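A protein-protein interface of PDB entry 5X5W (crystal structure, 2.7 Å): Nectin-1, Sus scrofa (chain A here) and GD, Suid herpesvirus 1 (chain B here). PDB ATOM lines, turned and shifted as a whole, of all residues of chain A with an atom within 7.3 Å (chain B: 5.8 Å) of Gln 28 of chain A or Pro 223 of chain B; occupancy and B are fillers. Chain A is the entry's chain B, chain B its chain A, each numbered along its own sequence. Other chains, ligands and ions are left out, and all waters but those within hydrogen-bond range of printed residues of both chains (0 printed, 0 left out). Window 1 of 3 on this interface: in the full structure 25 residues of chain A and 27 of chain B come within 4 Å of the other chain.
Of the printed residues of chain B, Asn 46 of chain A touches Trp 39 (3.6 Å). Printed residues of chain A within 4 Å of Met 218 of chain B: Asn 41 (3.0 Å) and Ile 44 (3.2 Å). Printed residues of chain A within 4 Å of Tyr 225 of chain B: Thr 27 (2.8 Å), Ala 91 (3.1 Å) and Thr 92 (3.2 Å). The nearest residue of chain B that does not touch Gln 28 of chain A is Thr 222 of chain B (4.4 Å).
The backbone carbonyl oxygen of Trp 134 of chain B lies within hydrogen-bond range of the backbone NH of Thr 222 of chain B, at 2.8 Å. N of Phe 224 of chain B is in hydrogen-bond range of O of Pro 132 of chain B, at 2.9 Å. OE1 of Glu 89 of chain A sits at hydrogen-bond distance from ND2 of Asn 97 of chain A (3.4 Å). The backbone carbonyl oxygen (O) of Gln 28 of chain A sits at hydrogen-bond distance from the backbone NH (N) of Ala 91 of chain A, 3.0 Å away. The side-chain amide oxygen (OD1) of Asn 46 of chain A sits close to the backbone carbonyl oxygen (O) of Thr 27 of chain A, at 3.2 Å. The backbone NH of Thr 27 of chain A lies within hydrogen-bond range of the backbone carbonyl oxygen of Ala 91 of chain A (2.8 Å).
Trp 39 of chain B touches Gln 28 of chain A. Thr 222 of chain B touches Asn 41 of chain A. CH2 of Trp 39 of chain B touches O of Ile 44 of chain A, at 3.9 Å. CE of Met 218 of chain B touches CD1 of Ile 44 of chain A (3.2 Å). Asn 46 of chain A touches Trp 39 of chain B. Met 49 of chain A touches Trp 39 of chain B (CE to CD1, 3.2 Å). Thr 131 of chain B touches Met 49 of chain A. Gly 50 of chain A touches Trp 39 of chain B (O to CH2, 3.5 Å). Phe 224 of chain B touches Asn 97 of chain A (CE2 to ND2, 3.5 Å).
The backbone carbonyl oxygen of Ala 91 of chain A lies within hydrogen-bond range of the side-chain hydroxyl of Tyr 225 of chain B (3.1 Å). OH of Tyr 225 of chain B lies close to O of Thr 92 of chain A (3.3 Å). The backbone carbonyl oxygen (O) of Leu 221 of chain B lies within hydrogen-bond range of the side-chain amide nitrogen (ND2) of Asn 41 of chain A, at 3.3 Å. O of Met 218 of chain B sits at hydrogen-bond distance from ND2 of Asn 41 of chain A, 3.0 Å away. OH of Tyr 225 of chain B sits at hydrogen-bond distance from OG1 of Thr 27 of chain A (2.8 Å). The side-chain amide nitrogen (NE2) of Gln 28 of chain A is in hydrogen-bond range of the backbone carbonyl oxygen (O) of Pro 223 of chain B (3.0 Å).
Of the 21 printed residues of chain A, 10 touch a printed residue of chain B. Hydrophobic or aromatic side chains of chain A within 4 Å of the printed part of chain B: Ile 44 and Met 49. Printed residues of chain B that touch a printed residue of chain A: Trp 39, Thr 131, Met 218, Leu 221, Thr 222, Pro 223, Phe 224 and Tyr 225. Hydrophobic or aromatic side chains of chain B that line the printed part of chain A: Trp 39, Met 218, Pro 223, Phe 224 and Tyr 225. Among the printed residues, 15 pairs touch across the chains.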
ATOM      1  N   LYS A  25      -4.833  -8.814 -15.376  1.00  0.00           N
ATOM      2  CA  LYS A  25      -4.128  -9.939 -14.862  1.00  0.00           C
ATOM      3  C   LYS A  25      -4.793 -11.067 -15.558  1.00  0.00           C
ATOM      4  O   LYS A  25      -5.969 -11.017 -15.777  1.00  0.00           O
ATOM      5  CB  LYS A  25      -4.403 -10.041 -13.381  1.00  0.00           C
ATOM      6  CG  LYS A  25      -3.456 -10.926 -12.602  1.00  0.00           C
ATOM      7  CD  LYS A  25      -3.698 -10.817 -11.107  1.00  0.00           C
ATOM      8  CE  LYS A  25      -3.857 -12.182 -10.476  1.00  0.00           C
ATOM      9  NZ  LYS A  25      -4.077 -12.104  -9.017  1.00  0.00           N
ATOM     10  N   ILE A  26      -4.038 -12.076 -15.946  1.00  0.00           N
ATOM     11  CA  ILE A  26      -4.635 -13.262 -16.471  1.00  0.00           C
ATOM     12  C   ILE A  26      -4.442 -14.250 -15.386  1.00  0.00           C
ATOM     13  O   ILE A  26      -3.343 -14.542 -15.028  1.00  0.00           O
ATOM     14  CB  ILE A  26      -3.943 -13.768 -17.716  1.00  0.00           C
ATOM     15  CG1 ILE A  26      -3.960 -12.714 -18.789  1.00  0.00           C
ATOM     16  CG2 ILE A  26      -4.673 -14.962 -18.242  1.00  0.00           C
ATOM     17  CD1 ILE A  26      -2.807 -11.760 -18.659  1.00  0.00           C
ATOM     18  N   THR A  27      -5.531 -14.746 -14.848  1.00  0.00           N
ATOM     19  CA  THR A  27      -5.498 -15.626 -13.687  1.00  0.00           C
ATOM     20  C   THR A  27      -5.492 -17.096 -14.082  1.00  0.00           C
ATOM     21  O   THR A  27      -4.800 -17.901 -13.464  1.00  0.00           O
ATOM     22  CB  THR A  27      -6.706 -15.369 -12.753  1.00  0.00           C
ATOM     23  OG1 THR A  27      -6.697 -14.003 -12.321  1.00  0.00           O
ATOM     24  CG2 THR A  27      -6.664 -16.283 -11.532  1.00  0.00           C
ATOM     25  N   GLN A  28      -6.249 -17.438 -15.120  1.00  0.00           N
ATOM     26  CA  GLN A  28      -6.564 -18.839 -15.379  1.00  0.00           C
ATOM     27  C   GLN A  28      -6.845 -19.150 -16.847  1.00  0.00           C
ATOM     28  O   GLN A  28      -7.328 -18.293 -17.590  1.00  0.00           O
ATOM     29  CB  GLN A  28      -7.775 -19.243 -14.532  1.00  0.00           C
ATOM     30  CG  GLN A  28      -7.785 -20.684 -14.092  1.00  0.00           C
ATOM     31  CD  GLN A  28      -8.994 -21.028 -13.246  1.00  0.00           C
ATOM     32  OE1 GLN A  28      -8.858 -21.429 -12.090  1.00  0.00           O
ATOM     33  NE2 GLN A  28     -10.182 -20.893 -13.824  1.00  0.00           N
ATOM     34  N   VAL A  29      -6.541 -20.382 -17.251  1.00  0.00           N
ATOM     35  CA  VAL A  29      -6.928 -20.894 -18.563  1.00  0.00           C
ATOM     36  C   VAL A  29      -7.696 -22.194 -18.396  1.00  0.00           C
ATOM     37  O   VAL A  29      -7.225 -23.111 -17.718  1.00  0.00           O
ATOM     38  CB  VAL A  29      -5.719 -21.179 -19.477  1.00  0.00           C
ATOM     39  CG1 VAL A  29      -6.191 -21.637 -20.841  1.00  0.00           C
ATOM     40  CG2 VAL A  29      -4.843 -19.965 -19.604  1.00  0.00           C
ATOM     41  N   THR A  30      -8.861 -22.286 -19.022  1.00  0.00           N
ATOM     42  CA  THR A  30      -9.629 -23.521 -18.992  1.00  0.00           C
ATOM     43  C   THR A  30      -9.937 -23.991 -20.405  1.00  0.00           C
ATOM     44  O   THR A  30     -10.438 -23.229 -21.227  1.00  0.00           O
ATOM     45  CB  THR A  30     -10.951 -23.358 -18.206  1.00  0.00           C
ATOM     46  OG1 THR A  30     -10.663 -23.043 -16.838  1.00  0.00           O
ATOM     47  CG2 THR A  30     -11.775 -24.637 -18.267  1.00  0.00           C
ATOM     48  N   ASN A  41     -15.356 -29.250 -18.950  1.00  0.00           N
ATOM     49  CA  ASN A  41     -14.002 -28.827 -18.974  1.00  0.00           C
ATOM     50  C   ASN A  41     -13.058 -29.948 -19.206  1.00  0.00           C
ATOM     51  O   ASN A  41     -13.227 -31.000 -18.688  1.00  0.00           O
ATOM     52  CB  ASN A  41     -13.666 -28.215 -17.650  1.00  0.00           C
ATOM     53  CG  ASN A  41     -14.469 -27.001 -17.339  1.00  0.00           C
ATOM     54  OD1 ASN A  41     -14.768 -26.204 -18.178  1.00  0.00           O
ATOM     55  ND2 ASN A  41     -14.783 -26.852 -16.110  1.00  0.00           N
ATOM     56  N   ILE A  44      -7.387 -27.399 -16.921  1.00  0.00           N
ATOM     57  CA  ILE A  44      -7.294 -26.088 -16.352  1.00  0.00           C
ATOM     58  C   ILE A  44      -5.894 -25.807 -15.868  1.00  0.00           C
ATOM     59  O   ILE A  44      -5.302 -26.643 -15.264  1.00  0.00           O
ATOM     60  CB  ILE A  44      -8.153 -25.991 -15.102  1.00  0.00           C
ATOM     61  CG1 ILE A  44      -9.441 -26.744 -15.250  1.00  0.00           C
ATOM     62  CG2 ILE A  44      -8.518 -24.568 -14.823  1.00  0.00           C
ATOM     63  CD1 ILE A  44      -9.955 -27.248 -13.942  1.00  0.00           C
ATOM     64  N   TYR A  45      -5.386 -24.608 -16.100  1.00  0.00           N
ATOM     65  CA  TYR A  45      -4.101 -24.214 -15.560  1.00  0.00           C
ATOM     66  C   TYR A  45      -4.178 -22.927 -14.773  1.00  0.00           C
ATOM     67  O   TYR A  45      -4.721 -21.962 -15.235  1.00  0.00           O
ATOM     68  CB  TYR A  45      -3.074 -24.059 -16.672  1.00  0.00           C
ATOM     69  CG  TYR A  45      -1.785 -23.437 -16.235  1.00  0.00           C
ATOM     70  CD1 TYR A  45      -0.994 -24.059 -15.336  1.00  0.00           C
ATOM     71  CD2 TYR A  45      -1.399 -22.209 -16.690  1.00  0.00           C
ATOM     72  CE1 TYR A  45       0.164 -23.496 -14.910  1.00  0.00           C
ATOM     73  CE2 TYR A  45      -0.245 -21.634 -16.264  1.00  0.00           C
ATOM     74  CZ  TYR A  45       0.534 -22.298 -15.378  1.00  0.00           C
ATOM     75  OH  TYR A  45       1.708 -21.766 -14.933  1.00  0.00           O
ATOM     76  N   ASN A  46      -3.571 -22.919 -13.598  1.00  0.00           N
ATOM     77  CA  ASN A  46      -3.497 -21.725 -12.786  1.00  0.00           C
ATOM     78  C   ASN A  46      -2.247 -21.681 -11.954  1.00  0.00           C
ATOM     79  O   ASN A  46      -2.105 -22.441 -11.027  1.00  0.00           O
ATOM     80  CB  ASN A  46      -4.701 -21.668 -11.875  1.00  0.00           C
ATOM     81  CG  ASN A  46      -4.751 -20.428 -11.060  1.00  0.00           C
ATOM     82  OD1 ASN A  46      -3.807 -19.689 -10.999  1.00  0.00           O
ATOM     83  ND2 ASN A  46      -5.839 -20.216 -10.403  1.00  0.00           N
ATOM     84  N   PRO A  47      -1.342 -20.779 -12.288  1.00  0.00           N
ATOM     85  CA  PRO A  47      -0.070 -20.620 -11.572  1.00  0.00           C
ATOM     86  C   PRO A  47      -0.247 -20.660 -10.055  1.00  0.00           C
ATOM     87  O   PRO A  47       0.674 -21.026  -9.325  1.00  0.00           O
ATOM     88  CB  PRO A  47       0.412 -19.244 -12.031  1.00  0.00           C
ATOM     89  CG  PRO A  47      -0.128 -19.125 -13.414  1.00  0.00           C
ATOM     90  CD  PRO A  47      -1.476 -19.803 -13.385  1.00  0.00           C
ATOM     91  N   ALA A  48      -1.441 -20.293  -9.601  1.00  0.00           N
ATOM     92  CA  ALA A  48      -1.789 -20.345  -8.188  1.00  0.00           C
ATOM     93  C   ALA A  48      -1.730 -21.770  -7.636  1.00  0.00           C
ATOM     94  O   ALA A  48      -1.065 -22.013  -6.629  1.00  0.00           O
ATOM     95  CB  ALA A  48      -3.169 -19.749  -7.969  1.00  0.00           C
ATOM     96  N   MET A  49      -2.413 -22.710  -8.288  1.00  0.00           N
ATOM     97  CA  MET A  49      -2.420 -24.097  -7.815  1.00  0.00           C
ATOM     98  C   MET A  49      -1.997 -25.129  -8.861  1.00  0.00           C
ATOM     99  O   MET A  49      -2.013 -26.329  -8.586  1.00  0.00           O
ATOM    100  CB  MET A  49      -3.804 -24.476  -7.280  1.00  0.00           C
ATOM    101  CG  MET A  49      -4.171 -23.776  -5.992  1.00  0.00           C
ATOM    102  SD  MET A  49      -5.235 -22.369  -6.317  1.00  0.00           S
ATOM    103  CE  MET A  49      -6.778 -23.210  -6.595  1.00  0.00           C
ATOM    104  N   GLY A  50      -1.627 -24.679 -10.056  1.00  0.00           N
ATOM    105  CA  GLY A  50      -1.057 -25.588 -11.038  1.00  0.00           C
ATOM    106  C   GLY A  50      -1.989 -26.113 -12.114  1.00  0.00           C
ATOM    107  O   GLY A  50      -2.710 -25.348 -12.758  1.00  0.00           O
ATOM    108  N   PHE A  68      -0.027 -18.630 -20.303  1.00  0.00           N
ATOM    109  CA  PHE A  68      -1.087 -17.960 -21.052  1.00  0.00           C
ATOM    110  C   PHE A  68      -0.530 -17.423 -22.358  1.00  0.00           C
ATOM    111  O   PHE A  68      -1.250 -17.253 -23.345  1.00  0.00           O
ATOM    112  CB  PHE A  68      -1.686 -16.824 -20.230  1.00  0.00           C
ATOM    113  CG  PHE A  68      -1.688 -17.088 -18.755  1.00  0.00           C
ATOM    114  CD1 PHE A  68      -0.712 -16.541 -17.938  1.00  0.00           C
ATOM    115  CD2 PHE A  68      -2.654 -17.895 -18.186  1.00  0.00           C
ATOM    116  CE1 PHE A  68      -0.713 -16.790 -16.582  1.00  0.00           C
ATOM    117  CE2 PHE A  68      -2.659 -18.148 -16.832  1.00  0.00           C
ATOM    118  CZ  PHE A  68      -1.689 -17.592 -16.030  1.00  0.00           C
ATOM    119  N   GLU A  89     -11.060 -20.729 -22.466  1.00  0.00           N
ATOM    120  CA  GLU A  89     -11.586 -19.685 -21.597  1.00  0.00           C
ATOM    121  C   GLU A  89     -10.529 -19.105 -20.658  1.00  0.00           C
ATOM    122  O   GLU A  89      -9.832 -19.839 -19.955  1.00  0.00           O
ATOM    123  CB  GLU A  89     -12.758 -20.223 -20.788  1.00  0.00           C
ATOM    124  CG  GLU A  89     -13.644 -19.144 -20.231  1.00  0.00           C
ATOM    125  CD  GLU A  89     -14.665 -19.695 -19.274  1.00  0.00           C
ATOM    126  OE1 GLU A  89     -14.375 -19.728 -18.057  1.00  0.00           O
ATOM    127  OE2 GLU A  89     -15.748 -20.102 -19.744  1.00  0.00           O
ATOM    128  N   PHE A  90     -10.419 -17.780 -20.658  1.00  0.00           N
ATOM    129  CA  PHE A  90      -9.449 -17.071 -19.829  1.00  0.00           C
ATOM    130  C   PHE A  90     -10.138 -16.275 -18.722  1.00  0.00           C
ATOM    131  O   PHE A  90     -11.025 -15.474 -18.999  1.00  0.00           O
ATOM    132  CB  PHE A  90      -8.612 -16.116 -20.682  1.00  0.00           C
ATOM    133  CG  PHE A  90      -7.634 -16.801 -21.598  1.00  0.00           C
ATOM    134  CD1 PHE A  90      -6.320 -16.995 -21.201  1.00  0.00           C
ATOM    135  CD2 PHE A  90      -8.014 -17.227 -22.864  1.00  0.00           C
ATOM    136  CE1 PHE A  90      -5.403 -17.611 -22.042  1.00  0.00           C
ATOM    137  CE2 PHE A  90      -7.095 -17.848 -23.712  1.00  0.00           C
ATOM    138  CZ  PHE A  90      -5.788 -18.035 -23.294  1.00  0.00           C
ATOM    139  N   ALA A  91      -9.726 -16.486 -17.477  1.00  0.00           N
ATOM    140  CA  ALA A  91     -10.224 -15.678 -16.369  1.00  0.00           C
ATOM    141  C   ALA A  91      -9.342 -14.451 -16.188  1.00  0.00           C
ATOM    142  O   ALA A  91      -8.262 -14.549 -15.606  1.00  0.00           O
ATOM    143  CB  ALA A  91     -10.267 -16.485 -15.086  1.00  0.00           C
ATOM    144  N   THR A  92      -9.790 -13.301 -16.687  1.00  0.00           N
ATOM    145  CA  THR A  92      -9.014 -12.069 -16.555  1.00  0.00           C
ATOM    146  C   THR A  92      -9.627 -11.109 -15.532  1.00  0.00           C
ATOM    147  O   THR A  92     -10.829 -11.150 -15.266  1.00  0.00           O
ATOM    148  CB  THR A  92      -8.871 -11.336 -17.911  1.00  0.00           C
ATOM    149  OG1 THR A  92     -10.162 -10.949 -18.399  1.00  0.00           O
ATOM    150  CG2 THR A  92      -8.204 -12.235 -18.929  1.00  0.00           C
ATOM    151  N   ASN A  97     -14.363 -13.271 -17.776  1.00  0.00           N
ATOM    152  CA  ASN A  97     -14.092 -14.373 -18.687  1.00  0.00           C
ATOM    153  C   ASN A  97     -14.031 -13.936 -20.138  1.00  0.00           C
ATOM    154  O   ASN A  97     -14.968 -13.335 -20.665  1.00  0.00           O
ATOM    155  CB  ASN A  97     -15.138 -15.471 -18.538  1.00  0.00           C
ATOM    156  CG  ASN A  97     -14.958 -16.269 -17.270  1.00  0.00           C
ATOM    157  OD1 ASN A  97     -15.928 -16.607 -16.590  1.00  0.00           O
ATOM    158  ND2 ASN A  97     -13.710 -16.567 -16.933  1.00  0.00           N
ATOM    159  N   ARG A  98     -12.929 -14.311 -20.776  1.00  0.00           N
ATOM    160  CA  ARG A  98     -12.646 -14.057 -22.174  1.00  0.00           C
ATOM    161  C   ARG A  98     -12.330 -15.368 -22.849  1.00  0.00           C
ATOM    162  O   ARG A  98     -11.512 -16.109 -22.371  1.00  0.00           O
ATOM    163  CB  ARG A  98     -11.422 -13.163 -22.270  1.00  0.00           C
ATOM    164  CG  ARG A  98     -11.539 -12.037 -23.264  1.00  0.00           C
ATOM    165  CD  ARG A  98     -11.544 -10.686 -22.584  1.00  0.00           C
ATOM    166  NE  ARG A  98     -12.895 -10.287 -22.220  1.00  0.00           N
ATOM    167  CZ  ARG A  98     -13.419  -9.089 -22.437  1.00  0.00           C
ATOM    168  NH1 ARG A  98     -12.715  -8.133 -23.018  1.00  0.00           N
ATOM    169  NH2 ARG A  98     -14.653  -8.844 -22.059  1.00  0.00           N
ATOM    170  N   TRP B  39      -8.140 -26.074  -4.921  1.00  0.00           N
ATOM    171  CA  TRP B  39      -9.227 -26.349  -5.851  1.00  0.00           C
ATOM    172  C   TRP B  39     -10.207 -27.327  -5.221  1.00  0.00           C
ATOM    173  O   TRP B  39     -11.403 -27.287  -5.504  1.00  0.00           O
ATOM    174  CB  TRP B  39      -8.697 -26.910  -7.178  1.00  0.00           C
ATOM    175  CG  TRP B  39      -8.454 -25.865  -8.238  1.00  0.00           C
ATOM    176  CD1 TRP B  39      -9.077 -24.651  -8.358  1.00  0.00           C
ATOM    177  CD2 TRP B  39      -7.518 -25.941  -9.318  1.00  0.00           C
ATOM    178  NE1 TRP B  39      -8.581 -23.969  -9.443  1.00  0.00           N
ATOM    179  CE2 TRP B  39      -7.626 -24.742 -10.051  1.00  0.00           C
ATOM    180  CE3 TRP B  39      -6.601 -26.908  -9.738  1.00  0.00           C
ATOM    181  CZ2 TRP B  39      -6.851 -24.487 -11.179  1.00  0.00           C
ATOM    182  CZ3 TRP B  39      -5.836 -26.652 -10.856  1.00  0.00           C
ATOM    183  CH2 TRP B  39      -5.965 -25.452 -11.562  1.00  0.00           C
ATOM    184  N   THR B 131     -11.530 -22.536  -4.144  1.00  0.00           N
ATOM    185  CA  THR B 131     -12.020 -21.493  -5.036  1.00  0.00           C
ATOM    186  C   THR B 131     -13.469 -21.823  -5.334  1.00  0.00           C
ATOM    187  O   THR B 131     -13.801 -23.001  -5.496  1.00  0.00           O
ATOM    188  CB  THR B 131     -11.235 -21.444  -6.347  1.00  0.00           C
ATOM    189  OG1 THR B 131     -11.262 -22.750  -6.946  1.00  0.00           O
ATOM    190  CG2 THR B 131      -9.783 -21.055  -6.085  1.00  0.00           C
ATOM    191  N   PRO B 132     -14.345 -20.803  -5.389  1.00  0.00           N
ATOM    192  CA  PRO B 132     -15.720 -21.072  -5.820  1.00  0.00           C
ATOM    193  C   PRO B 132     -15.731 -21.716  -7.202  1.00  0.00           C
ATOM    194  O   PRO B 132     -14.930 -21.338  -8.061  1.00  0.00           O
ATOM    195  CB  PRO B 132     -16.365 -19.680  -5.860  1.00  0.00           C
ATOM    196  CG  PRO B 132     -15.537 -18.849  -4.942  1.00  0.00           C
ATOM    197  CD  PRO B 132     -14.133 -19.371  -5.113  1.00  0.00           C
ATOM    198  N   MET B 133     -16.665 -22.602  -7.443  1.00  0.00           N
ATOM    199  CA  MET B 133     -16.790 -23.227  -8.716  1.00  0.00           C
ATOM    200  C   MET B 133     -18.045 -22.761  -9.335  1.00  0.00           C
ATOM    201  O   MET B 133     -19.092 -22.966  -8.830  1.00  0.00           O
ATOM    202  CB  MET B 133     -16.830 -24.726  -8.582  1.00  0.00           C
ATOM    203  CG  MET B 133     -15.793 -25.266  -7.648  1.00  0.00           C
ATOM    204  SD  MET B 133     -14.278 -25.433  -8.516  1.00  0.00           S
ATOM    205  CE  MET B 133     -13.100 -25.216  -7.256  1.00  0.00           C
ATOM    206  N   TRP B 134     -17.917 -22.118 -10.467  1.00  0.00           N
ATOM    207  CA  TRP B 134     -19.083 -21.509 -11.096  1.00  0.00           C
ATOM    208  C   TRP B 134     -19.445 -22.134 -12.430  1.00  0.00           C
ATOM    209  O   TRP B 134     -18.613 -22.749 -13.103  1.00  0.00           O
ATOM    210  CB  TRP B 134     -18.864 -20.015 -11.311  1.00  0.00           C
ATOM    211  CG  TRP B 134     -19.152 -19.147 -10.130  1.00  0.00           C
ATOM    212  CD1 TRP B 134     -18.279 -18.783  -9.147  1.00  0.00           C
ATOM    213  CD2 TRP B 134     -20.390 -18.496  -9.829  1.00  0.00           C
ATOM    214  NE1 TRP B 134     -18.904 -17.953  -8.243  1.00  0.00           N
ATOM    215  CE2 TRP B 134     -20.200 -17.760  -8.642  1.00  0.00           C
ATOM    216  CE3 TRP B 134     -21.644 -18.468 -10.447  1.00  0.00           C
ATOM    217  CZ2 TRP B 134     -21.215 -17.006  -8.060  1.00  0.00           C
ATOM    218  CZ3 TRP B 134     -22.651 -17.716  -9.868  1.00  0.00           C
ATOM    219  CH2 TRP B 134     -22.431 -16.996  -8.686  1.00  0.00           C
ATOM    220  N   MET B 218     -15.259 -30.164 -10.932  1.00  0.00           N
ATOM    221  CA  MET B 218     -14.486 -29.348 -11.862  1.00  0.00           C
ATOM    222  C   MET B 218     -14.672 -29.743 -13.328  1.00  0.00           C
ATOM    223  O   MET B 218     -14.108 -29.103 -14.222  1.00  0.00           O
ATOM    224  CB  MET B 218     -13.001 -29.407 -11.509  1.00  0.00           C
ATOM    225  CG  MET B 218     -12.670 -28.996 -10.091  1.00  0.00           C
ATOM    226  SD  MET B 218     -10.886 -29.001  -9.811  1.00  0.00           S
ATOM    227  CE  MET B 218     -10.367 -27.592 -10.782  1.00  0.00           C
ATOM    228  N   LEU B 221     -18.301 -27.605 -13.441  1.00  0.00           N
ATOM    229  CA  LEU B 221     -18.159 -26.261 -12.880  1.00  0.00           C
ATOM    230  C   LEU B 221     -16.705 -25.797 -13.000  1.00  0.00           C
ATOM    231  O   LEU B 221     -15.791 -26.618 -13.004  1.00  0.00           O
ATOM    232  CB  LEU B 221     -18.618 -26.220 -11.420  1.00  0.00           C
ATOM    233  CG  LEU B 221     -20.115 -26.420 -11.151  1.00  0.00           C
ATOM    234  CD1 LEU B 221     -20.396 -26.538  -9.660  1.00  0.00           C
ATOM    235  CD2 LEU B 221     -20.929 -25.287 -11.754  1.00  0.00           C
ATOM    236  N   THR B 222     -16.471 -24.512 -13.123  1.00  0.00           N
ATOM    237  CA  THR B 222     -15.117 -24.074 -13.311  1.00  0.00           C
ATOM    238  C   THR B 222     -14.683 -23.108 -12.226  1.00  0.00           C
ATOM    239  O   THR B 222     -15.444 -22.333 -11.767  1.00  0.00           O
ATOM    240  CB  THR B 222     -14.806 -23.645 -14.770  1.00  0.00           C
ATOM    241  OG1 THR B 222     -14.176 -22.389 -14.785  1.00  0.00           O
ATOM    242  CG2 THR B 222     -15.994 -23.574 -15.636  1.00  0.00           C
ATOM    243  N   PRO B 223     -13.451 -23.206 -11.789  1.00  0.00           N
ATOM    244  CA  PRO B 223     -12.947 -22.377 -10.683  1.00  0.00           C
ATOM    245  C   PRO B 223     -12.972 -20.889 -11.020  1.00  0.00           C
ATOM    246  O   PRO B 223     -12.612 -20.518 -12.141  1.00  0.00           O
ATOM    247  CB  PRO B 223     -11.499 -22.857 -10.503  1.00  0.00           C
ATOM    248  CG  PRO B 223     -11.426 -24.153 -11.193  1.00  0.00           C
ATOM    249  CD  PRO B 223     -12.420 -24.117 -12.304  1.00  0.00           C
ATOM    250  N   PHE B 224     -13.371 -20.042 -10.075  1.00  0.00           N
ATOM    251  CA  PHE B 224     -13.423 -18.610 -10.356  1.00  0.00           C
ATOM    252  C   PHE B 224     -12.826 -17.765  -9.226  1.00  0.00           C
ATOM    253  O   PHE B 224     -12.063 -18.263  -8.402  1.00  0.00           O
ATOM    254  CB  PHE B 224     -14.863 -18.186 -10.642  1.00  0.00           C
ATOM    255  CG  PHE B 224     -14.964 -16.985 -11.528  1.00  0.00           C
ATOM    256  CD1 PHE B 224     -15.747 -15.895 -11.173  1.00  0.00           C
ATOM    257  CD2 PHE B 224     -14.241 -16.931 -12.711  1.00  0.00           C
ATOM    258  CE1 PHE B 224     -15.824 -14.784 -11.997  1.00  0.00           C
ATOM    259  CE2 PHE B 224     -14.312 -15.826 -13.533  1.00  0.00           C
ATOM    260  CZ  PHE B 224     -15.104 -14.749 -13.176  1.00  0.00           C
ATOM    261  N   TYR B 225     -13.151 -16.478  -9.200  1.00  0.00           N
ATOM    262  CA  TYR B 225     -12.638 -15.605  -8.152  1.00  0.00           C
ATOM    263  C   TYR B 225     -13.483 -15.705  -6.883  1.00  0.00           C
ATOM    264  O   TYR B 225     -14.697 -15.931  -6.934  1.00  0.00           O
ATOM    265  CB  TYR B 225     -12.595 -14.145  -8.619  1.00  0.00           C
ATOM    266  CG  TYR B 225     -11.691 -13.866  -9.800  1.00  0.00           C
ATOM    267  CD1 TYR B 225     -10.320 -14.070  -9.721  1.00  0.00           C
ATOM    268  CD2 TYR B 225     -12.210 -13.368 -10.990  1.00  0.00           C
ATOM    269  CE1 TYR B 225      -9.490 -13.804 -10.803  1.00  0.00           C
ATOM    270  CE2 TYR B 225     -11.394 -13.098 -12.072  1.00  0.00           C
ATOM    271  CZ  TYR B 225     -10.035 -13.317 -11.976  1.00  0.00           C
ATOM    272  OH  TYR B 225      -9.225 -13.050 -13.058  1.00  0.00           O
